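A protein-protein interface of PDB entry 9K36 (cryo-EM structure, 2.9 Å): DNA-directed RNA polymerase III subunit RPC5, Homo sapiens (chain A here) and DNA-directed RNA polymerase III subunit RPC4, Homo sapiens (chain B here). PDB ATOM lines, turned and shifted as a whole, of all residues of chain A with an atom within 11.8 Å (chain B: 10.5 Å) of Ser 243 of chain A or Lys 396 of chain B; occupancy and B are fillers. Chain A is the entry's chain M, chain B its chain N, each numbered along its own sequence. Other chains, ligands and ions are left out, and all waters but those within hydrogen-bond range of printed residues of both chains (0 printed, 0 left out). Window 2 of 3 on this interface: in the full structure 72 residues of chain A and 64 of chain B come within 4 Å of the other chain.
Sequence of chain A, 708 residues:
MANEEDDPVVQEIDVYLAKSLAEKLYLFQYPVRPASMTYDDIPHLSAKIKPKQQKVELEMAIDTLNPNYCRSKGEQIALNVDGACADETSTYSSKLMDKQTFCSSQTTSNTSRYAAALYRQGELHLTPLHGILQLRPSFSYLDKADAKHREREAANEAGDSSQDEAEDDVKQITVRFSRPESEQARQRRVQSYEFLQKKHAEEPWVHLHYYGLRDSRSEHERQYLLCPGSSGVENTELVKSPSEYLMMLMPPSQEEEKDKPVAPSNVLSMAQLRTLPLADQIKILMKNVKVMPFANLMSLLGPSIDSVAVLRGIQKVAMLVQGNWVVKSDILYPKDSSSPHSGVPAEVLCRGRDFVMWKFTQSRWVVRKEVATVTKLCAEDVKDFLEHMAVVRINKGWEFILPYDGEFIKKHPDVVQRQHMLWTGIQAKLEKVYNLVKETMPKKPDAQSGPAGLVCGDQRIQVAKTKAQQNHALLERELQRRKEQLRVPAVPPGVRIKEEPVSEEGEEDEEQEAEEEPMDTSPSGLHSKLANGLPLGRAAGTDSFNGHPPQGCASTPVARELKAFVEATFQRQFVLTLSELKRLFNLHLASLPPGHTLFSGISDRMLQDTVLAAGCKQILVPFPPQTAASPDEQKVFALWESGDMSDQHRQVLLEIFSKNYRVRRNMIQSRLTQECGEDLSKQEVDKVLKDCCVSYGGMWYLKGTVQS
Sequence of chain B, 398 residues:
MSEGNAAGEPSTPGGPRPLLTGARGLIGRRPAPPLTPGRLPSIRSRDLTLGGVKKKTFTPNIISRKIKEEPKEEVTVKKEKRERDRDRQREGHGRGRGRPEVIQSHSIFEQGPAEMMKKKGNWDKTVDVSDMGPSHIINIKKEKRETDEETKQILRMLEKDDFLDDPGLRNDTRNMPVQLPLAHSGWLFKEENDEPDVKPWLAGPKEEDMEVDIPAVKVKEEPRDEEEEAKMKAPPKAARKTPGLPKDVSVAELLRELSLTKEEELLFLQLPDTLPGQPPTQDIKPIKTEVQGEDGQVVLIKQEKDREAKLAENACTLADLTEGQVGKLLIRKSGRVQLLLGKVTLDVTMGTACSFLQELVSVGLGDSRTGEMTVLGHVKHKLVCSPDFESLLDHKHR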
ATOM      1  N   LEU A 238      -9.176 -33.691   6.074  1.00  0.00           N
ATOM      2  CA  LEU A 238      -9.245 -32.426   6.809  1.00  0.00           C
ATOM      3  C   LEU A 238      -9.241 -31.236   5.849  1.00  0.00           C
ATOM      4  O   LEU A 238      -8.543 -30.241   6.053  1.00  0.00           O
ATOM      5  CB  LEU A 238      -8.109 -32.313   7.830  1.00  0.00           C
ATOM      6  CG  LEU A 238      -8.033 -33.405   8.903  1.00  0.00           C
ATOM      7  CD1 LEU A 238      -6.830 -33.181   9.806  1.00  0.00           C
ATOM      8  CD2 LEU A 238      -9.317 -33.454   9.718  1.00  0.00           C
ATOM      9  N   VAL A 239     -10.039 -31.350   4.783  1.00  0.00           N
ATOM     10  CA  VAL A 239     -10.121 -30.335   3.744  1.00  0.00           C
ATOM     11  C   VAL A 239     -11.546 -29.838   3.538  1.00  0.00           C
ATOM     12  O   VAL A 239     -11.836 -29.210   2.519  1.00  0.00           O
ATOM     13  CB  VAL A 239      -9.530 -30.851   2.417  1.00  0.00           C
ATOM     14  CG1 VAL A 239      -8.040 -31.122   2.564  1.00  0.00           C
ATOM     15  CG2 VAL A 239     -10.262 -32.104   1.963  1.00  0.00           C
ATOM     16  N   LYS A 240     -12.445 -30.105   4.481  1.00  0.00           N
ATOM     17  CA  LYS A 240     -13.823 -29.654   4.340  1.00  0.00           C
ATOM     18  C   LYS A 240     -13.940 -28.170   4.665  1.00  0.00           C
ATOM     19  O   LYS A 240     -13.202 -27.636   5.497  1.00  0.00           O
ATOM     20  CB  LYS A 240     -14.748 -30.470   5.242  1.00  0.00           C
ATOM     21  CG  LYS A 240     -14.951 -31.903   4.774  1.00  0.00           C
ATOM     22  CD  LYS A 240     -16.177 -32.531   5.418  1.00  0.00           C
ATOM     23  CE  LYS A 240     -16.471 -33.892   4.809  1.00  0.00           C
ATOM     24  NZ  LYS A 240     -17.749 -34.467   5.310  1.00  0.00           N
ATOM     25  N   SER A 241     -14.881 -27.505   3.994  1.00  0.00           N
ATOM     26  CA  SER A 241     -15.095 -26.083   4.196  1.00  0.00           C
ATOM     27  C   SER A 241     -15.709 -25.823   5.571  1.00  0.00           C
ATOM     28  O   SER A 241     -16.257 -26.730   6.198  1.00  0.00           O
ATOM     29  CB  SER A 241     -16.001 -25.527   3.099  1.00  0.00           C
ATOM     30  OG  SER A 241     -17.286 -26.116   3.149  1.00  0.00           O
ATOM     31  N   PRO A 242     -15.610 -24.582   6.069  1.00  0.00           N
ATOM     32  CA  PRO A 242     -16.252 -24.264   7.358  1.00  0.00           C
ATOM     33  C   PRO A 242     -17.746 -24.547   7.383  1.00  0.00           C
ATOM     34  O   PRO A 242     -18.271 -24.972   8.421  1.00  0.00           O
ATOM     35  CB  PRO A 242     -15.950 -22.770   7.529  1.00  0.00           C
ATOM     36  CG  PRO A 242     -14.681 -22.563   6.775  1.00  0.00           C
ATOM     37  CD  PRO A 242     -14.772 -23.472   5.583  1.00  0.00           C
ATOM     38  N   SER A 243     -18.444 -24.322   6.268  1.00  0.00           N
ATOM     39  CA  SER A 243     -19.871 -24.628   6.222  1.00  0.00           C
ATOM     40  C   SER A 243     -20.116 -26.125   6.373  1.00  0.00           C
ATOM     41  O   SER A 243     -21.021 -26.543   7.107  1.00  0.00           O
ATOM     42  CB  SER A 243     -20.477 -24.111   4.918  1.00  0.00           C
ATOM     43  OG  SER A 243     -21.865 -24.390   4.856  1.00  0.00           O
ATOM     44  N   GLU A 244     -19.317 -26.946   5.688  1.00  0.00           N
ATOM     45  CA  GLU A 244     -19.458 -28.394   5.820  1.00  0.00           C
ATOM     46  C   GLU A 244     -19.147 -28.851   7.239  1.00  0.00           C
ATOM     47  O   GLU A 244     -19.832 -29.727   7.781  1.00  0.00           O
ATOM     48  CB  GLU A 244     -18.550 -29.102   4.813  1.00  0.00           C
ATOM     49  CG  GLU A 244     -18.949 -28.886   3.360  1.00  0.00           C
ATOM     50  CD  GLU A 244     -17.978 -29.526   2.387  1.00  0.00           C
ATOM     51  OE1 GLU A 244     -16.939 -30.050   2.840  1.00  0.00           O
ATOM     52  OE2 GLU A 244     -18.257 -29.508   1.170  1.00  0.00           O
ATOM     53  N   TYR A 245     -18.122 -28.264   7.864  1.00  0.00           N
ATOM     54  CA  TYR A 245     -17.804 -28.612   9.245  1.00  0.00           C
ATOM     55  C   TYR A 245     -18.947 -28.245  10.182  1.00  0.00           C
ATOM     56  O   TYR A 245     -19.308 -29.028  11.071  1.00  0.00           O
ATOM     57  CB  TYR A 245     -16.512 -27.915   9.677  1.00  0.00           C
ATOM     58  CG  TYR A 245     -15.950 -28.413  10.991  1.00  0.00           C
ATOM     59  CD1 TYR A 245     -16.265 -29.678  11.469  1.00  0.00           C
ATOM     60  CD2 TYR A 245     -15.109 -27.613  11.754  1.00  0.00           C
ATOM     61  CE1 TYR A 245     -15.755 -30.135  12.668  1.00  0.00           C
ATOM     62  CE2 TYR A 245     -14.595 -28.064  12.956  1.00  0.00           C
ATOM     63  CZ  TYR A 245     -14.921 -29.325  13.409  1.00  0.00           C
ATOM     64  OH  TYR A 245     -14.412 -29.776  14.603  1.00  0.00           O
ATOM     65  N   LEU A 246     -19.531 -27.057  10.001  1.00  0.00           N
ATOM     66  CA  LEU A 246     -20.643 -26.637  10.846  1.00  0.00           C
ATOM     67  C   LEU A 246     -21.855 -27.540  10.650  1.00  0.00           C
ATOM     68  O   LEU A 246     -22.561 -27.863  11.614  1.00  0.00           O
ATOM     69  CB  LEU A 246     -21.001 -25.180  10.557  1.00  0.00           C
ATOM     70  CG  LEU A 246     -22.116 -24.563  11.403  1.00  0.00           C
ATOM     71  CD1 LEU A 246     -21.774 -24.640  12.882  1.00  0.00           C
ATOM     72  CD2 LEU A 246     -22.368 -23.124  10.983  1.00  0.00           C
ATOM     73  N   MET A 247     -22.116 -27.955   9.408  1.00  0.00           N
ATOM     74  CA  MET A 247     -23.210 -28.891   9.162  1.00  0.00           C
ATOM     75  C   MET A 247     -22.925 -30.246   9.796  1.00  0.00           C
ATOM     76  O   MET A 247     -23.848 -30.931  10.253  1.00  0.00           O
ATOM     77  CB  MET A 247     -23.452 -29.041   7.659  1.00  0.00           C
ATOM     78  CG  MET A 247     -23.954 -27.782   6.966  1.00  0.00           C
ATOM     79  SD  MET A 247     -25.531 -27.179   7.605  1.00  0.00           S
ATOM     80  CE  MET A 247     -24.990 -25.792   8.601  1.00  0.00           C
ATOM     81  N   MET A 248     -21.653 -30.650   9.832  1.00  0.00           N
ATOM     82  CA  MET A 248     -21.298 -31.931  10.431  1.00  0.00           C
ATOM     83  C   MET A 248     -21.489 -31.907  11.944  1.00  0.00           C
ATOM     84  O   MET A 248     -22.165 -32.774  12.507  1.00  0.00           O
ATOM     85  CB  MET A 248     -19.854 -32.292  10.079  1.00  0.00           C
ATOM     86  CG  MET A 248     -19.351 -33.557  10.758  1.00  0.00           C
ATOM     87  SD  MET A 248     -17.618 -33.899  10.403  1.00  0.00           S
ATOM     88  CE  MET A 248     -17.667 -34.075   8.623  1.00  0.00           C
ATOM     89  N   LEU A 249     -20.900 -30.918  12.620  1.00  0.00           N
ATOM     90  CA  LEU A 249     -20.981 -30.861  14.076  1.00  0.00           C
ATOM     91  C   LEU A 249     -22.337 -30.382  14.580  1.00  0.00           C
ATOM     92  O   LEU A 249     -22.576 -30.422  15.793  1.00  0.00           O
ATOM     93  CB  LEU A 249     -19.865 -29.972  14.638  1.00  0.00           C
ATOM     94  CG  LEU A 249     -19.715 -28.529  14.147  1.00  0.00           C
ATOM     95  CD1 LEU A 249     -20.567 -27.564  14.955  1.00  0.00           C
ATOM     96  CD2 LEU A 249     -18.254 -28.102  14.179  1.00  0.00           C
ATOM     97  N   MET A 250     -23.223 -29.934  13.692  1.00  0.00           N
ATOM     98  CA  MET A 250     -24.594 -29.564  14.042  1.00  0.00           C
ATOM     99  C   MET A 250     -25.542 -30.180  13.021  1.00  0.00           C
ATOM    100  O   MET A 250     -26.056 -29.492  12.132  1.00  0.00           O
ATOM    101  CB  MET A 250     -24.763 -28.046  14.100  1.00  0.00           C
ATOM    102  CG  MET A 250     -24.118 -27.392  15.308  1.00  0.00           C
ATOM    103  SD  MET A 250     -24.750 -28.034  16.869  1.00  0.00           S
ATOM    104  CE  MET A 250     -26.485 -27.611  16.733  1.00  0.00           C
ATOM    105  N   PRO A 251     -25.798 -31.488  13.122  1.00  0.00           N
ATOM    106  CA  PRO A 251     -26.693 -32.127  12.166  1.00  0.00           C
ATOM    107  C   PRO A 251     -28.130 -31.705  12.408  1.00  0.00           C
ATOM    108  O   PRO A 251     -28.530 -31.439  13.554  1.00  0.00           O
ATOM    109  CB  PRO A 251     -26.496 -33.627  12.444  1.00  0.00           C
ATOM    110  CG  PRO A 251     -26.096 -33.679  13.879  1.00  0.00           C
ATOM    111  CD  PRO A 251     -25.276 -32.440  14.120  1.00  0.00           C
ATOM    112  N   PRO A 252     -28.944 -31.623  11.358  1.00  0.00           N
ATOM    113  CA  PRO A 252     -30.351 -31.252  11.545  1.00  0.00           C
ATOM    114  C   PRO A 252     -31.116 -32.320  12.310  1.00  0.00           C
ATOM    115  O   PRO A 252     -30.725 -33.488  12.358  1.00  0.00           O
ATOM    116  CB  PRO A 252     -30.877 -31.114  10.110  1.00  0.00           C
ATOM    117  CG  PRO A 252     -29.655 -30.942   9.261  1.00  0.00           C
ATOM    118  CD  PRO A 252     -28.586 -31.741   9.935  1.00  0.00           C
ATOM    119  N   ARG A 274     -37.542 -18.294   0.518  1.00  0.00           N
ATOM    120  CA  ARG A 274     -36.407 -18.482  -0.381  1.00  0.00           C
ATOM    121  C   ARG A 274     -36.140 -19.950  -0.688  1.00  0.00           C
ATOM    122  O   ARG A 274     -35.548 -20.253  -1.730  1.00  0.00           O
ATOM    123  CB  ARG A 274     -35.155 -17.837   0.214  1.00  0.00           C
ATOM    124  CG  ARG A 274     -35.248 -16.324   0.352  1.00  0.00           C
ATOM    125  CD  ARG A 274     -33.987 -15.746   0.976  1.00  0.00           C
ATOM    126  NE  ARG A 274     -34.058 -14.296   1.116  1.00  0.00           N
ATOM    127  CZ  ARG A 274     -33.092 -13.544   1.633  1.00  0.00           C
ATOM    128  NH1 ARG A 274     -31.970 -14.107   2.063  1.00  0.00           N
ATOM    129  NH2 ARG A 274     -33.243 -12.230   1.719  1.00  0.00           N
ATOM    130  N   THR B 274     -16.110 -34.130  16.661  1.00  0.00           N
ATOM    131  CA  THR B 274     -15.924 -34.344  15.232  1.00  0.00           C
ATOM    132  C   THR B 274     -14.865 -33.385  14.712  1.00  0.00           C
ATOM    133  O   THR B 274     -14.951 -32.175  14.941  1.00  0.00           O
ATOM    134  CB  THR B 274     -17.236 -34.144  14.468  1.00  0.00           C
ATOM    135  OG1 THR B 274     -17.696 -32.799  14.649  1.00  0.00           O
ATOM    136  CG2 THR B 274     -18.303 -35.110  14.968  1.00  0.00           C
ATOM    137  N   PRO B 276     -12.798 -31.526  11.509  1.00  0.00           N
ATOM    138  CA  PRO B 276     -13.224 -31.048  10.186  1.00  0.00           C
ATOM    139  C   PRO B 276     -12.652 -31.870   9.043  1.00  0.00           C
ATOM    140  O   PRO B 276     -11.902 -31.347   8.215  1.00  0.00           O
ATOM    141  CB  PRO B 276     -12.692 -29.610  10.153  1.00  0.00           C
ATOM    142  CG  PRO B 276     -11.511 -29.636  11.062  1.00  0.00           C
ATOM    143  CD  PRO B 276     -11.879 -30.583  12.169  1.00  0.00           C
ATOM    144  N   GLY B 277     -13.007 -33.152   8.984  1.00  0.00           N
ATOM    145  CA  GLY B 277     -12.520 -34.027   7.938  1.00  0.00           C
ATOM    146  C   GLY B 277     -13.480 -35.170   7.696  1.00  0.00           C
ATOM    147  O   GLY B 277     -14.541 -35.264   8.316  1.00  0.00           O
ATOM    148  N   GLU B 313     -21.691 -38.527   7.093  1.00  0.00           N
ATOM    149  CA  GLU B 313     -21.426 -37.389   7.977  1.00  0.00           C
ATOM    150  C   GLU B 313     -21.284 -37.838   9.431  1.00  0.00           C
ATOM    151  O   GLU B 313     -21.763 -37.180  10.358  1.00  0.00           O
ATOM    152  CB  GLU B 313     -22.507 -36.315   7.841  1.00  0.00           C
ATOM    153  CG  GLU B 313     -22.595 -35.679   6.461  1.00  0.00           C
ATOM    154  CD  GLU B 313     -23.452 -36.480   5.496  1.00  0.00           C
ATOM    155  OE1 GLU B 313     -24.400 -37.149   5.957  1.00  0.00           O
ATOM    156  OE2 GLU B 313     -23.177 -36.438   4.278  1.00  0.00           O
ATOM    157  N   LYS B 343      -9.035 -25.991   6.470  1.00  0.00           N
ATOM    158  CA  LYS B 343      -9.712 -24.758   6.081  1.00  0.00           C
ATOM    159  C   LYS B 343     -10.230 -23.991   7.294  1.00  0.00           C
ATOM    160  O   LYS B 343     -10.334 -22.761   7.245  1.00  0.00           O
ATOM    161  CB  LYS B 343     -10.853 -25.066   5.113  1.00  0.00           C
ATOM    162  CG  LYS B 343     -10.393 -25.604   3.769  1.00  0.00           C
ATOM    163  CD  LYS B 343     -11.565 -25.809   2.826  1.00  0.00           C
ATOM    164  CE  LYS B 343     -11.096 -26.263   1.453  1.00  0.00           C
ATOM    165  NZ  LYS B 343     -10.342 -27.545   1.514  1.00  0.00           N
ATOM    166  N   VAL B 344     -10.555 -24.690   8.376  1.00  0.00           N
ATOM    167  CA  VAL B 344     -11.072 -24.054   9.575  1.00  0.00           C
ATOM    168  C   VAL B 344      -9.939 -23.905  10.581  1.00  0.00           C
ATOM    169  O   VAL B 344      -8.874 -24.519  10.462  1.00  0.00           O
ATOM    170  CB  VAL B 344     -12.247 -24.850  10.188  1.00  0.00           C
ATOM    171  CG1 VAL B 344     -13.216 -25.282   9.102  1.00  0.00           C
ATOM    172  CG2 VAL B 344     -11.732 -26.046  10.969  1.00  0.00           C
ATOM    173  N   THR B 345     -10.170 -23.064  11.589  1.00  0.00           N
ATOM    174  CA  THR B 345      -9.196 -22.813  12.645  1.00  0.00           C
ATOM    175  C   THR B 345      -9.902 -22.881  13.991  1.00  0.00           C
ATOM    176  O   THR B 345     -10.835 -22.112  14.246  1.00  0.00           O
ATOM    177  CB  THR B 345      -8.518 -21.450  12.470  1.00  0.00           C
ATOM    178  OG1 THR B 345      -9.517 -20.427  12.360  1.00  0.00           O
ATOM    179  CG2 THR B 345      -7.646 -21.438  11.221  1.00  0.00           C
ATOM    180  N   ASP B 388     -14.006 -22.402  16.552  1.00  0.00           N
ATOM    181  CA  ASP B 388     -14.255 -20.962  16.545  1.00  0.00           C
ATOM    182  C   ASP B 388     -15.601 -20.723  15.864  1.00  0.00           C
ATOM    183  O   ASP B 388     -15.692 -20.404  14.678  1.00  0.00           O
ATOM    184  CB  ASP B 388     -13.124 -20.221  15.845  1.00  0.00           C
ATOM    185  CG  ASP B 388     -13.214 -18.715  16.020  1.00  0.00           C
ATOM    186  OD1 ASP B 388     -14.077 -18.253  16.794  1.00  0.00           O
ATOM    187  OD2 ASP B 388     -12.420 -17.994  15.379  1.00  0.00           O
ATOM    188  N   PHE B 389     -16.669 -20.885  16.651  1.00  0.00           N
ATOM    189  CA  PHE B 389     -18.019 -20.812  16.097  1.00  0.00           C
ATOM    190  C   PHE B 389     -18.331 -19.434  15.531  1.00  0.00           C
ATOM    191  O   PHE B 389     -19.097 -19.322  14.568  1.00  0.00           O
ATOM    192  CB  PHE B 389     -19.047 -21.188  17.163  1.00  0.00           C
ATOM    193  CG  PHE B 389     -19.042 -22.646  17.524  1.00  0.00           C
ATOM    194  CD1 PHE B 389     -19.690 -23.571  16.724  1.00  0.00           C
ATOM    195  CD2 PHE B 389     -18.396 -23.090  18.664  1.00  0.00           C
ATOM    196  CE1 PHE B 389     -19.689 -24.911  17.052  1.00  0.00           C
ATOM    197  CE2 PHE B 389     -18.390 -24.431  18.996  1.00  0.00           C
ATOM    198  CZ  PHE B 389     -19.040 -25.343  18.190  1.00  0.00           C
ATOM    199  N   GLU B 390     -17.754 -18.377  16.107  1.00  0.00           N
ATOM    200  CA  GLU B 390     -18.015 -17.034  15.601  1.00  0.00           C
ATOM    201  C   GLU B 390     -17.536 -16.883  14.161  1.00  0.00           C
ATOM    202  O   GLU B 390     -18.258 -16.345  13.312  1.00  0.00           O
ATOM    203  CB  GLU B 390     -17.350 -15.992  16.500  1.00  0.00           C
ATOM    204  CG  GLU B 390     -17.650 -14.550  16.114  1.00  0.00           C
ATOM    205  CD  GLU B 390     -17.041 -13.552  17.078  1.00  0.00           C
ATOM    206  OE1 GLU B 390     -16.304 -13.980  17.993  1.00  0.00           O
ATOM    207  OE2 GLU B 390     -17.300 -12.339  16.925  1.00  0.00           O
ATOM    208  N   SER B 391     -16.324 -17.361  13.868  1.00  0.00           N
ATOM    209  CA  SER B 391     -15.808 -17.290  12.504  1.00  0.00           C
ATOM    210  C   SER B 391     -16.603 -18.190  11.566  1.00  0.00           C
ATOM    211  O   SER B 391     -16.875 -17.814  10.418  1.00  0.00           O
ATOM    212  CB  SER B 391     -14.327 -17.663  12.481  1.00  0.00           C
ATOM    213  OG  SER B 391     -14.128 -18.988  12.940  1.00  0.00           O
ATOM    214  N   LEU B 392     -16.986 -19.380  12.034  1.00  0.00           N
ATOM    215  CA  LEU B 392     -17.787 -20.277  11.207  1.00  0.00           C
ATOM    216  C   LEU B 392     -19.148 -19.676  10.887  1.00  0.00           C
ATOM    217  O   LEU B 392     -19.728 -19.978   9.839  1.00  0.00           O
ATOM    218  CB  LEU B 392     -17.955 -21.627  11.904  1.00  0.00           C
ATOM    219  CG  LEU B 392     -16.674 -22.349  12.328  1.00  0.00           C
ATOM    220  CD1 LEU B 392     -16.998 -23.700  12.943  1.00  0.00           C
ATOM    221  CD2 LEU B 392     -15.720 -22.504  11.154  1.00  0.00           C
ATOM    222  N   LEU B 393     -19.671 -18.823  11.771  1.00  0.00           N
ATOM    223  CA  LEU B 393     -20.959 -18.189  11.518  1.00  0.00           C
ATOM    224  C   LEU B 393     -20.816 -16.976  10.605  1.00  0.00           C
ATOM    225  O   LEU B 393     -21.604 -16.803   9.669  1.00  0.00           O
ATOM    226  CB  LEU B 393     -21.624 -17.798  12.839  1.00  0.00           C
ATOM    227  CG  LEU B 393     -22.176 -18.957  13.667  1.00  0.00           C
ATOM    228  CD1 LEU B 393     -22.848 -18.450  14.933  1.00  0.00           C
ATOM    229  CD2 LEU B 393     -23.143 -19.795  12.844  1.00  0.00           C
ATOM    230  N   ASP B 394     -19.818 -16.125  10.856  1.00  0.00           N
ATOM    231  CA  ASP B 394     -19.644 -14.952  10.004  1.00  0.00           C
ATOM    232  C   ASP B 394     -19.099 -15.309   8.626  1.00  0.00           C
ATOM    233  O   ASP B 394     -19.149 -14.472   7.720  1.00  0.00           O
ATOM    234  CB  ASP B 394     -18.740 -13.909  10.678  1.00  0.00           C
ATOM    235  CG  ASP B 394     -17.360 -14.446  11.027  1.00  0.00           C
ATOM    236  OD1 ASP B 394     -16.681 -15.011  10.145  1.00  0.00           O
ATOM    237  OD2 ASP B 394     -16.936 -14.264  12.188  1.00  0.00           O
ATOM    238  N   HIS B 395     -18.580 -16.527   8.451  1.00  0.00           N
ATOM    239  CA  HIS B 395     -18.105 -16.945   7.136  1.00  0.00           C
ATOM    240  C   HIS B 395     -19.268 -17.131   6.169  1.00  0.00           C
ATOM    241  O   HIS B 395     -19.264 -16.584   5.060  1.00  0.00           O
ATOM    242  CB  HIS B 395     -17.290 -18.231   7.262  1.00  0.00           C
ATOM    243  CG  HIS B 395     -16.684 -18.692   5.973  1.00  0.00           C
ATOM    244  ND1 HIS B 395     -17.283 -19.631   5.163  1.00  0.00           N
ATOM    245  CD2 HIS B 395     -15.529 -18.343   5.357  1.00  0.00           C
ATOM    246  CE1 HIS B 395     -16.524 -19.841   4.100  1.00  0.00           C
ATOM    247  NE2 HIS B 395     -15.454 -19.071   4.193  1.00  0.00           N
ATOM    248  N   LYS B 396     -20.272 -17.904   6.574  1.00  0.00           N
ATOM    249  CA  LYS B 396     -21.461 -18.114   5.755  1.00  0.00           C
ATOM    250  C   LYS B 396     -22.724 -18.052   6.610  1.00  0.00           C
ATOM    251  O   LYS B 396     -23.410 -19.058   6.793  1.00  0.00           O
ATOM    252  CB  LYS B 396     -21.390 -19.454   5.021  1.00  0.00           C
ATOM    253  CG  LYS B 396     -20.372 -19.498   3.891  1.00  0.00           C
ATOM    254  CD  LYS B 396     -20.421 -20.827   3.157  1.00  0.00           C
ATOM    255  CE  LYS B 396     -19.426 -20.864   2.008  1.00  0.00           C
ATOM    256  NZ  LYS B 396     -19.482 -22.157   1.273  1.00  0.00           N
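The side-chain hydroxyl (OG) of Ser 241 of chain A lies close to the backbone NH (N) of Glu 244 of chain A (3.4 Å).
Among the printed residues, merely in contact across the chains: Leu 238 of chain A with Pro 276 of chain B, Leu 238 of chain A with Gly 277 of chain B, Val 239 of chain A with Pro 276 of chain B, Lys 240 of chain A with Pro 276 of chain B, Lys 240 of chain A with Lys 343 of chain B, Ser 241 of chain A with Lys 343 of chain B, Pro 242 of chain A with Val 344 of chain B, Pro 242 of chain A with Leu 392 of chain B, Ser 243 of chain A with Lys 396 of chain B, Tyr 245 of chain A with Pro 276 of chain B, Tyr 245 of chain A with Val 344 of chain B, Leu 246 of chain A with Leu 393 of chain B, Met 248 of chain A with Gly 277 of chain B, Leu 249 of chain A with Thr 274 of chain B and Leu 249 of chain A with Phe 389 of chain B.
Of the 16 printed residues of chain A, 10 touch a printed residue of chain B.
Printed residues of chain A that touch a printed residue of chain B: Leu 238, Val 239, Lys 240, Ser 241, Pro 242, Ser 243, Tyr 245, Leu 246, Met 248 and Leu 249.
Along chain A the printed residues that touch a printed residue of chain B span positions 238 to 249.
Printed residues of chain B that touch a printed residue of chain A: Thr 274, Pro 276, Gly 277, Lys 343, Val 344, Phe 389, Leu 392, Leu 393 and Lys 396.
Hydrophobic or aromatic side chains of chain B that line the printed part of chain A: Pro 276, Val 344, Phe 389, Leu 392 and Leu 393.
Among the printed residues, 17 pairs touch across the chains.
Of chain A, only Ser 243 comes within 4 Å of Lys 396 of chain B.
Ser 241 of chain A touches just one residue of chain B: Lys 343.
Pro 242 of chain A touches just these residues of chain B: Val 344 and Leu 392.
Met 247 of chain A touches none of the printed residues of chain B.
Of chain A, only Pro 242 comes within 4 Å of Leu 392 of chain B.
No residue of chain A comes within 4 Å of Asp 394 of chain B.
No residue of chain A comes within 4 Å of His 395 of chain B.
Of the printed residues of chain B, Leu 238 of chain A touches Pro 276 and Gly 277.
Of the printed residues of chain A, Lys 343 of chain B touches Val 239, Lys 240 and Ser 241.
Printed residues of chain B within 4 Å of Leu 249 of chain A: Thr 274 (3.6 Å) and Phe 389 (3.5 Å).
Of the printed residues of chain A, Phe 389 of chain B touches Leu 249 (3.5 Å).
Of the printed residues of chain B, Lys 240 of chain A touches Pro 276 (3.97 Å) and Lys 343 (3.5 Å).
The nearest residue of chain B that does not touch Ser 243 of chain A is His 395 of chain B (5.0 Å).
O of Val 239 of chain A is in hydrogen-bond range of NZ of Lys 343 of chain B (2.5 Å).
The side-chain hydroxyl (OH) of Tyr 245 of chain A is in hydrogen-bond range of the backbone carbonyl oxygen (O) of Thr 274 of chain B, at 2.5 Å.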
